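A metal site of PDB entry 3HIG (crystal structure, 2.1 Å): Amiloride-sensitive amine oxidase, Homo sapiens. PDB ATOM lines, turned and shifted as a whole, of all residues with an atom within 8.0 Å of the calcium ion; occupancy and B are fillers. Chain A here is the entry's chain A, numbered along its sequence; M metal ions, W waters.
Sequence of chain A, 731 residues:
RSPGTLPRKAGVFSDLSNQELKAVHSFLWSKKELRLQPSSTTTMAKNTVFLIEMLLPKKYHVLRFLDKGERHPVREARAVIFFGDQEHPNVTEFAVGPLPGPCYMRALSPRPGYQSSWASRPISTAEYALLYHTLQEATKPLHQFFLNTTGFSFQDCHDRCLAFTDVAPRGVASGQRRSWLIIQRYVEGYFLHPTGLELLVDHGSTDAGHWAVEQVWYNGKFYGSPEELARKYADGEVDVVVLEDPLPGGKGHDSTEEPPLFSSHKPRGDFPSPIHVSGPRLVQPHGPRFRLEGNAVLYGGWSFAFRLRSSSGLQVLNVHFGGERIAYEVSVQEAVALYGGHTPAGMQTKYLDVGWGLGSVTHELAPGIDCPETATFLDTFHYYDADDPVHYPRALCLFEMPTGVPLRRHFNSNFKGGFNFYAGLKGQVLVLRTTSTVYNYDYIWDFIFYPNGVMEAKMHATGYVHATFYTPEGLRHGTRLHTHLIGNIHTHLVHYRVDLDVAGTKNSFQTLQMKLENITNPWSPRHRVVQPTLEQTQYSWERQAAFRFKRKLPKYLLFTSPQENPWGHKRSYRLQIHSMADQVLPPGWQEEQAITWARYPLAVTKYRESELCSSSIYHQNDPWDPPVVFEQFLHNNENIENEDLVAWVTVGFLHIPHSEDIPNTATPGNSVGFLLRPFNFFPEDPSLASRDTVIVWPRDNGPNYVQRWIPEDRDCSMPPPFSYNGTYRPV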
ATOM      1  N   LYS A  59      -7.725   7.240  -3.765  1.00  0.00           N
ATOM      2  CA  LYS A  59      -6.308   7.596  -3.963  1.00  0.00           C
ATOM      3  C   LYS A  59      -6.081   8.308  -5.287  1.00  0.00           C
ATOM      4  O   LYS A  59      -5.315   9.282  -5.375  1.00  0.00           O
ATOM      5  CB  LYS A  59      -5.408   6.340  -3.806  1.00  0.00           C
ATOM      6  CG  LYS A  59      -3.887   6.543  -3.943  1.00  0.00           C
ATOM      7  CD  LYS A  59      -3.155   5.265  -3.508  1.00  0.00           C
ATOM      8  CE  LYS A  59      -1.653   5.301  -3.755  1.00  0.00           C
ATOM      9  NZ  LYS A  59      -0.918   3.992  -3.427  1.00  0.00           N
ATOM     10  N   ARG A 325       8.078  11.102  -2.557  1.00  0.00           N
ATOM     11  CA  ARG A 325       7.213  10.205  -1.806  1.00  0.00           C
ATOM     12  C   ARG A 325       7.870   8.847  -1.548  1.00  0.00           C
ATOM     13  O   ARG A 325       8.552   8.275  -2.426  1.00  0.00           O
ATOM     14  CB  ARG A 325       5.864  10.031  -2.519  1.00  0.00           C
ATOM     15  CG  ARG A 325       4.838   9.261  -1.703  1.00  0.00           C
ATOM     16  CD  ARG A 325       3.453   9.275  -2.341  1.00  0.00           C
ATOM     17  NE  ARG A 325       2.841  10.602  -2.305  1.00  0.00           N
ATOM     18  CZ  ARG A 325       2.519  11.341  -3.375  1.00  0.00           C
ATOM     19  NH1 ARG A 325       2.736  10.892  -4.612  1.00  0.00           N
ATOM     20  NH2 ARG A 325       1.989  12.538  -3.208  1.00  0.00           N
ATOM     21  N   ILE A 326       7.674   8.351  -0.320  1.00  0.00           N
ATOM     22  CA  ILE A 326       8.088   7.027   0.150  1.00  0.00           C
ATOM     23  C   ILE A 326       6.871   6.110   0.384  1.00  0.00           C
ATOM     24  O   ILE A 326       6.895   4.915   0.057  1.00  0.00           O
ATOM     25  CB  ILE A 326       8.810   7.140   1.512  1.00  0.00           C
ATOM     26  CG1 ILE A 326       9.984   8.121   1.445  1.00  0.00           C
ATOM     27  CG2 ILE A 326       9.256   5.768   2.010  1.00  0.00           C
ATOM     28  CD1 ILE A 326      10.761   8.045   0.153  1.00  0.00           C
ATOM     29  N   ALA A 327       5.837   6.675   1.003  1.00  0.00           N
ATOM     30  CA  ALA A 327       4.622   5.942   1.425  1.00  0.00           C
ATOM     31  C   ALA A 327       3.385   6.796   1.331  1.00  0.00           C
ATOM     32  O   ALA A 327       3.346   7.913   1.873  1.00  0.00           O
ATOM     33  CB  ALA A 327       4.766   5.488   2.877  1.00  0.00           C
ATOM     34  N   TYR A 328       2.346   6.288   0.670  1.00  0.00           N
ATOM     35  CA  TYR A 328       1.048   6.951   0.681  1.00  0.00           C
ATOM     36  C   TYR A 328       0.317   6.821   2.043  1.00  0.00           C
ATOM     37  O   TYR A 328      -0.371   7.750   2.482  1.00  0.00           O
ATOM     38  CB  TYR A 328       0.148   6.420  -0.450  1.00  0.00           C
ATOM     39  CG  TYR A 328      -1.146   7.168  -0.545  1.00  0.00           C
ATOM     40  CD1 TYR A 328      -1.189   8.439  -1.139  1.00  0.00           C
ATOM     41  CD2 TYR A 328      -2.334   6.626  -0.057  1.00  0.00           C
ATOM     42  CE1 TYR A 328      -2.371   9.144  -1.222  1.00  0.00           C
ATOM     43  CE2 TYR A 328      -3.542   7.340  -0.145  1.00  0.00           C
ATOM     44  CZ  TYR A 328      -3.541   8.593  -0.724  1.00  0.00           C
ATOM     45  OH  TYR A 328      -4.691   9.326  -0.806  1.00  0.00           O
ATOM     46  N   GLU A 329       0.456   5.665   2.689  1.00  0.00           N
ATOM     47  CA  GLU A 329      -0.215   5.364   3.960  1.00  0.00           C
ATOM     48  C   GLU A 329       0.570   4.323   4.753  1.00  0.00           C
ATOM     49  O   GLU A 329       1.047   3.329   4.202  1.00  0.00           O
ATOM     50  CB  GLU A 329      -1.637   4.849   3.689  1.00  0.00           C
ATOM     51  CG  GLU A 329      -2.469   4.550   4.935  1.00  0.00           C
ATOM     52  CD  GLU A 329      -3.680   3.657   4.649  1.00  0.00           C
ATOM     53  OE1 GLU A 329      -3.979   3.430   3.443  1.00  0.00           O
ATOM     54  OE2 GLU A 329      -4.335   3.177   5.616  1.00  0.00           O
ATOM     55  N   ARG A 497      -0.928  -1.809   7.748  1.00  0.00           N
ATOM     56  CA  ARG A 497      -0.979  -1.600   6.297  1.00  0.00           C
ATOM     57  C   ARG A 497       0.095  -0.613   5.936  1.00  0.00           C
ATOM     58  O   ARG A 497       0.172   0.467   6.519  1.00  0.00           O
ATOM     59  CB  ARG A 497      -2.320  -1.055   5.863  1.00  0.00           C
ATOM     60  CG  ARG A 497      -2.433  -0.713   4.408  1.00  0.00           C
ATOM     61  CD  ARG A 497      -3.792  -0.077   4.148  1.00  0.00           C
ATOM     62  NE  ARG A 497      -3.915   0.508   2.806  1.00  0.00           N
ATOM     63  CZ  ARG A 497      -4.345  -0.131   1.725  1.00  0.00           C
ATOM     64  NH1 ARG A 497      -4.682  -1.410   1.773  1.00  0.00           N
ATOM     65  NH2 ARG A 497      -4.410   0.510   0.566  1.00  0.00           N
ATOM     66  N   VAL A 498       0.893  -0.959   4.933  1.00  0.00           N
ATOM     67  CA  VAL A 498       2.042  -0.174   4.547  1.00  0.00           C
ATOM     68  C   VAL A 498       2.039   0.057   3.041  1.00  0.00           C
ATOM     69  O   VAL A 498       2.605  -0.720   2.250  1.00  0.00           O
ATOM     70  CB  VAL A 498       3.346  -0.817   5.000  1.00  0.00           C
ATOM     71  CG1 VAL A 498       4.487   0.162   4.827  1.00  0.00           C
ATOM     72  CG2 VAL A 498       3.221  -1.329   6.489  1.00  0.00           C
ATOM     73  N   ASP A 499       1.341   1.112   2.630  1.00  0.00           N
ATOM     74  CA  ASP A 499       1.162   1.389   1.209  1.00  0.00           C
ATOM     75  C   ASP A 499       2.350   2.239   0.779  1.00  0.00           C
ATOM     76  O   ASP A 499       2.267   3.461   0.722  1.00  0.00           O
ATOM     77  CB  ASP A 499      -0.175   2.074   0.958  1.00  0.00           C
ATOM     78  CG  ASP A 499      -0.421   2.430  -0.531  1.00  0.00           C
ATOM     79  OD1 ASP A 499       0.382   2.041  -1.405  1.00  0.00           O
ATOM     80  OD2 ASP A 499      -1.417   3.125  -0.844  1.00  0.00           O
ATOM     81  N   LEU A 500       3.472   1.594   0.503  1.00  0.00           N
ATOM     82  CA  LEU A 500       4.648   2.277  -0.001  1.00  0.00           C
ATOM     83  C   LEU A 500       4.389   2.637  -1.451  1.00  0.00           C
ATOM     84  O   LEU A 500       3.850   1.830  -2.189  1.00  0.00           O
ATOM     85  CB  LEU A 500       5.918   1.429   0.092  1.00  0.00           C
ATOM     86  CG  LEU A 500       6.310   1.038   1.508  1.00  0.00           C
ATOM     87  CD1 LEU A 500       7.243  -0.151   1.461  1.00  0.00           C
ATOM     88  CD2 LEU A 500       6.935   2.217   2.285  1.00  0.00           C
ATOM     89  N   ASP A 501       4.770   3.877  -1.787  1.00  0.00           N
ATOM     90  CA  ASP A 501       4.798   4.387  -3.138  1.00  0.00           C
ATOM     91  C   ASP A 501       6.226   4.922  -3.323  1.00  0.00           C
ATOM     92  O   ASP A 501       6.456   6.126  -3.265  1.00  0.00           O
ATOM     93  CB  ASP A 501       3.789   5.530  -3.284  1.00  0.00           C
ATOM     94  CG  ASP A 501       2.350   5.050  -3.409  1.00  0.00           C
ATOM     95  OD1 ASP A 501       2.076   3.819  -3.406  1.00  0.00           O
ATOM     96  OD2 ASP A 501       1.483   5.925  -3.573  1.00  0.00           O
ATOM     97  N   VAL A 502       7.176   4.009  -3.524  1.00  0.00           N
ATOM     98  CA  VAL A 502       8.595   4.365  -3.504  1.00  0.00           C
ATOM     99  C   VAL A 502       8.949   5.218  -4.734  1.00  0.00           C
ATOM    100  O   VAL A 502       8.874   4.767  -5.880  1.00  0.00           O
ATOM    101  CB  VAL A 502       9.507   3.108  -3.368  1.00  0.00           C
ATOM    102  CG1 VAL A 502      10.982   3.509  -3.404  1.00  0.00           C
ATOM    103  CG2 VAL A 502       9.137   2.291  -2.075  1.00  0.00           C
ATOM    104  N   GLY A 504       7.116   7.353  -6.056  1.00  0.00           N
ATOM    105  CA  GLY A 504       5.998   7.182  -7.017  1.00  0.00           C
ATOM    106  C   GLY A 504       5.213   5.881  -6.811  1.00  0.00           C
ATOM    107  O   GLY A 504       5.640   4.973  -6.090  1.00  0.00           O
ATOM    108  N   THR A 505       4.062   5.770  -7.502  1.00  0.00           N
ATOM    109  CA  THR A 505       3.122   4.689  -7.291  1.00  0.00           C
ATOM    110  C   THR A 505       3.605   3.311  -7.794  1.00  0.00           C
ATOM    111  O   THR A 505       3.329   2.305  -7.173  1.00  0.00           O
ATOM    112  CB  THR A 505       1.796   5.088  -7.961  1.00  0.00           C
ATOM    113  OG1 THR A 505       1.764   6.521  -8.074  1.00  0.00           O
ATOM    114  CG2 THR A 505       0.612   4.637  -7.149  1.00  0.00           C
ATOM    115  N   LYS A 506       4.326   3.272  -8.928  1.00  0.00           N
ATOM    116  CA  LYS A 506       4.693   1.977  -9.548  1.00  0.00           C
ATOM    117  C   LYS A 506       6.007   1.395  -9.044  1.00  0.00           C
ATOM    118  O   LYS A 506       7.091   1.927  -9.299  1.00  0.00           O
ATOM    119  CB  LYS A 506       4.717   2.026 -11.078  1.00  0.00           C
ATOM    120  CG  LYS A 506       3.363   2.392 -11.742  1.00  0.00           C
ATOM    121  CD  LYS A 506       2.186   1.550 -11.270  1.00  0.00           C
ATOM    122  CE  LYS A 506       0.860   2.009 -11.884  1.00  0.00           C
ATOM    123  NZ  LYS A 506       0.763   1.648 -13.334  1.00  0.00           N
ATOM    124  N   ASN A 507       5.861   0.292  -8.325  1.00  0.00           N
ATOM    125  CA  ASN A 507       6.970  -0.383  -7.709  1.00  0.00           C
ATOM    126  C   ASN A 507       7.002  -1.885  -8.058  1.00  0.00           C
ATOM    127  O   ASN A 507       6.042  -2.454  -8.645  1.00  0.00           O
ATOM    128  CB  ASN A 507       6.891  -0.231  -6.180  1.00  0.00           C
ATOM    129  CG  ASN A 507       6.906   1.235  -5.707  1.00  0.00           C
ATOM    130  OD1 ASN A 507       6.248   1.593  -4.696  1.00  0.00           O
ATOM    131  ND2 ASN A 507       7.660   2.096  -6.417  1.00  0.00           N
ATOM    132  N   PHE A 559      11.286  -2.828  -1.656  1.00  0.00           N
ATOM    133  CA  PHE A 559      10.270  -2.262  -2.502  1.00  0.00           C
ATOM    134  C   PHE A 559      10.985  -1.243  -3.364  1.00  0.00           C
ATOM    135  O   PHE A 559      11.569  -0.277  -2.853  1.00  0.00           O
ATOM    136  CB  PHE A 559       9.162  -1.676  -1.632  1.00  0.00           C
ATOM    137  CG  PHE A 559       8.438  -2.744  -0.883  1.00  0.00           C
ATOM    138  CD1 PHE A 559       8.934  -3.234   0.304  1.00  0.00           C
ATOM    139  CD2 PHE A 559       7.315  -3.353  -1.442  1.00  0.00           C
ATOM    140  CE1 PHE A 559       8.303  -4.276   0.975  1.00  0.00           C
ATOM    141  CE2 PHE A 559       6.678  -4.408  -0.805  1.00  0.00           C
ATOM    142  CZ  PHE A 559       7.179  -4.862   0.418  1.00  0.00           C
ATOM    143  N   THR A 605       0.201  -7.021  -1.743  1.00  0.00           N
ATOM    144  CA  THR A 605      -0.964  -7.056  -2.618  1.00  0.00           C
ATOM    145  C   THR A 605      -0.932  -5.910  -3.608  1.00  0.00           C
ATOM    146  O   THR A 605      -0.248  -4.886  -3.390  1.00  0.00           O
ATOM    147  CB  THR A 605      -2.315  -7.026  -1.838  1.00  0.00           C
ATOM    148  OG1 THR A 605      -2.442  -5.805  -1.100  1.00  0.00           O
ATOM    149  CG2 THR A 605      -2.403  -8.236  -0.902  1.00  0.00           C
ATOM    150  N   LYS A 606      -1.661  -6.080  -4.692  1.00  0.00           N
ATOM    151  CA  LYS A 606      -1.952  -4.976  -5.613  1.00  0.00           C
ATOM    152  C   LYS A 606      -3.023  -4.057  -5.019  1.00  0.00           C
ATOM    153  O   LYS A 606      -4.058  -4.526  -4.529  1.00  0.00           O
ATOM    154  CB  LYS A 606      -2.369  -5.512  -6.970  1.00  0.00           C
ATOM    155  CG  LYS A 606      -2.887  -4.458  -7.943  1.00  0.00           C
ATOM    156  CD  LYS A 606      -3.013  -5.057  -9.342  1.00  0.00           C
ATOM    157  CE  LYS A 606      -3.666  -4.096 -10.287  1.00  0.00           C
ATOM    158  NZ  LYS A 606      -3.338  -4.547 -11.660  1.00  0.00           N
ATOM    159  N   TYR A 607      -2.757  -2.751  -5.046  1.00  0.00           N
ATOM    160  CA  TYR A 607      -3.671  -1.719  -4.520  1.00  0.00           C
ATOM    161  C   TYR A 607      -5.073  -1.815  -5.145  1.00  0.00           C
ATOM    162  O   TYR A 607      -5.211  -1.999  -6.361  1.00  0.00           O
ATOM    163  CB  TYR A 607      -3.140  -0.311  -4.756  1.00  0.00           C
ATOM    164  CG  TYR A 607      -4.045   0.752  -4.185  1.00  0.00           C
ATOM    165  CD1 TYR A 607      -5.121   1.264  -4.898  1.00  0.00           C
ATOM    166  CD2 TYR A 607      -3.842   1.245  -2.896  1.00  0.00           C
ATOM    167  CE1 TYR A 607      -5.979   2.230  -4.342  1.00  0.00           C
ATOM    168  CE2 TYR A 607      -4.677   2.208  -2.343  1.00  0.00           C
ATOM    169  CZ  TYR A 607      -5.731   2.694  -3.060  1.00  0.00           C
ATOM    170  OH  TYR A 607      -6.536   3.643  -2.494  1.00  0.00           O
ATOM    171  N   GLU A 643       3.613  -2.230 -10.356  1.00  0.00           N
ATOM    172  CA  GLU A 643       2.233  -1.939  -9.947  1.00  0.00           C
ATOM    173  C   GLU A 643       2.264  -1.088  -8.679  1.00  0.00           C
ATOM    174  O   GLU A 643       3.328  -0.887  -8.049  1.00  0.00           O
ATOM    175  CB  GLU A 643       1.429  -3.219  -9.687  1.00  0.00           C
ATOM    176  CG  GLU A 643       1.275  -4.168 -10.883  1.00  0.00           C
ATOM    177  CD  GLU A 643       0.151  -3.786 -11.838  1.00  0.00           C
ATOM    178  OE1 GLU A 643      -0.928  -3.379 -11.375  1.00  0.00           O
ATOM    179  OE2 GLU A 643       0.339  -3.923 -13.052  1.00  0.00           O
ATOM    180  N   ASP A 644       1.092  -0.571  -8.328  1.00  0.00           N
ATOM    181  CA  ASP A 644       0.885   0.056  -7.037  1.00  0.00           C
ATOM    182  C   ASP A 644       0.743  -1.062  -6.016  1.00  0.00           C
ATOM    183  O   ASP A 644      -0.269  -1.755  -5.975  1.00  0.00           O
ATOM    184  CB  ASP A 644      -0.371   0.952  -7.076  1.00  0.00           C
ATOM    185  CG  ASP A 644      -0.525   1.777  -5.798  1.00  0.00           C
ATOM    186  OD1 ASP A 644       0.186   1.468  -4.816  1.00  0.00           O
ATOM    187  OD2 ASP A 644      -1.375   2.689  -5.753  1.00  0.00           O
ATOM    188  N   LEU A 645       1.762  -1.235  -5.176  1.00  0.00           N
ATOM    189  CA  LEU A 645       1.824  -2.317  -4.210  1.00  0.00           C
ATOM    190  C   LEU A 645       1.478  -1.834  -2.803  1.00  0.00           C
ATOM    191  O   LEU A 645       1.663  -0.643  -2.467  1.00  0.00           O
ATOM    192  CB  LEU A 645       3.222  -2.966  -4.161  1.00  0.00           C
ATOM    193  CG  LEU A 645       3.818  -3.468  -5.486  1.00  0.00           C
ATOM    194  CD1 LEU A 645       5.253  -4.102  -5.256  1.00  0.00           C
ATOM    195  CD2 LEU A 645       2.834  -4.444  -6.174  1.00  0.00           C
ATOM    196  N   VAL A 646       0.995  -2.761  -2.001  1.00  0.00           N
ATOM    197  CA  VAL A 646       0.746  -2.551  -0.588  1.00  0.00           C
ATOM    198  C   VAL A 646       1.405  -3.703   0.160  1.00  0.00           C
ATOM    199  O   VAL A 646       1.154  -4.842  -0.140  1.00  0.00           O
ATOM    200  CB  VAL A 646      -0.760  -2.529  -0.297  1.00  0.00           C
ATOM    201  CG1 VAL A 646      -1.002  -2.286   1.177  1.00  0.00           C
ATOM    202  CG2 VAL A 646      -1.458  -1.446  -1.154  1.00  0.00           C
ATOM    203  N   ALA A 647       2.269  -3.382   1.120  1.00  0.00           N
ATOM    204  CA  ALA A 647       2.833  -4.348   2.046  1.00  0.00           C
ATOM    205  C   ALA A 647       1.929  -4.436   3.282  1.00  0.00           C
ATOM    206  O   ALA A 647       1.425  -3.430   3.762  1.00  0.00           O
ATOM    207  CB  ALA A 647       4.233  -3.920   2.473  1.00  0.00           C
HETATM  208 CA    CA M   1       1.778   1.535  -3.173  1.00  0.00          CA
HETATM  209  O   HOH W   1       3.508   1.099  -4.941  1.00  0.00           O
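NZ of Lys 59 touches the calcium ion, 3.7 Å away. Within 4 Å of the calcium ion: Lys 59, Asp 499, Leu 500, Asp 501, Asp 644 and Leu 645.
The calcium ion is bound by the side-chain carboxylate of Asp 644 (2.3 Å), the backbone carbonyl oxygen of Leu 645 (2.3 Å), the side-chain carboxylate of Asp 499 (2.3 Å), the backbone carbonyl oxygen of Leu 500 (2.3 Å), the side-chain carboxylate of Asp 501 (2.3 Å) and water W1 (2.5 Å).
Water W1 lies within hydrogen-bond range of O of Thr 505 (2.5 Å), OD1 of Asn 507 (2.8 Å) and N of Leu 645 (2.9 Å).
The side-chain carboxylate (OD2) of Asp 644 lies within salt-bridge range of the side-chain amino group (NZ) of Lys 59 (2.7 Å). The backbone carbonyl oxygen (O) of Asp 644 is in hydrogen-bond range of the backbone NH (N) of Tyr 607 (2.8 Å). NZ of Lys 59 is in salt-bridge range of OD2 of Asp 499. The backbone NH (N) of Tyr 328 is in hydrogen-bond range of the backbone carbonyl oxygen (O) of Asp 499 (2.8 Å). N of Asp 499 is in hydrogen-bond range of O of Glu 329 (2.7 Å). The backbone carbonyl oxygen (O) of Leu 500 lies close to the side-chain amide oxygen (OD1) of Asn 507 (3.5 Å). OD2 of Asp 501 is in salt-bridge range of NZ of Lys 59 (3.1 Å). The backbone NH of Asp 501 lies within hydrogen-bond range of the backbone carbonyl oxygen of Ile 326 (3.0 Å).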
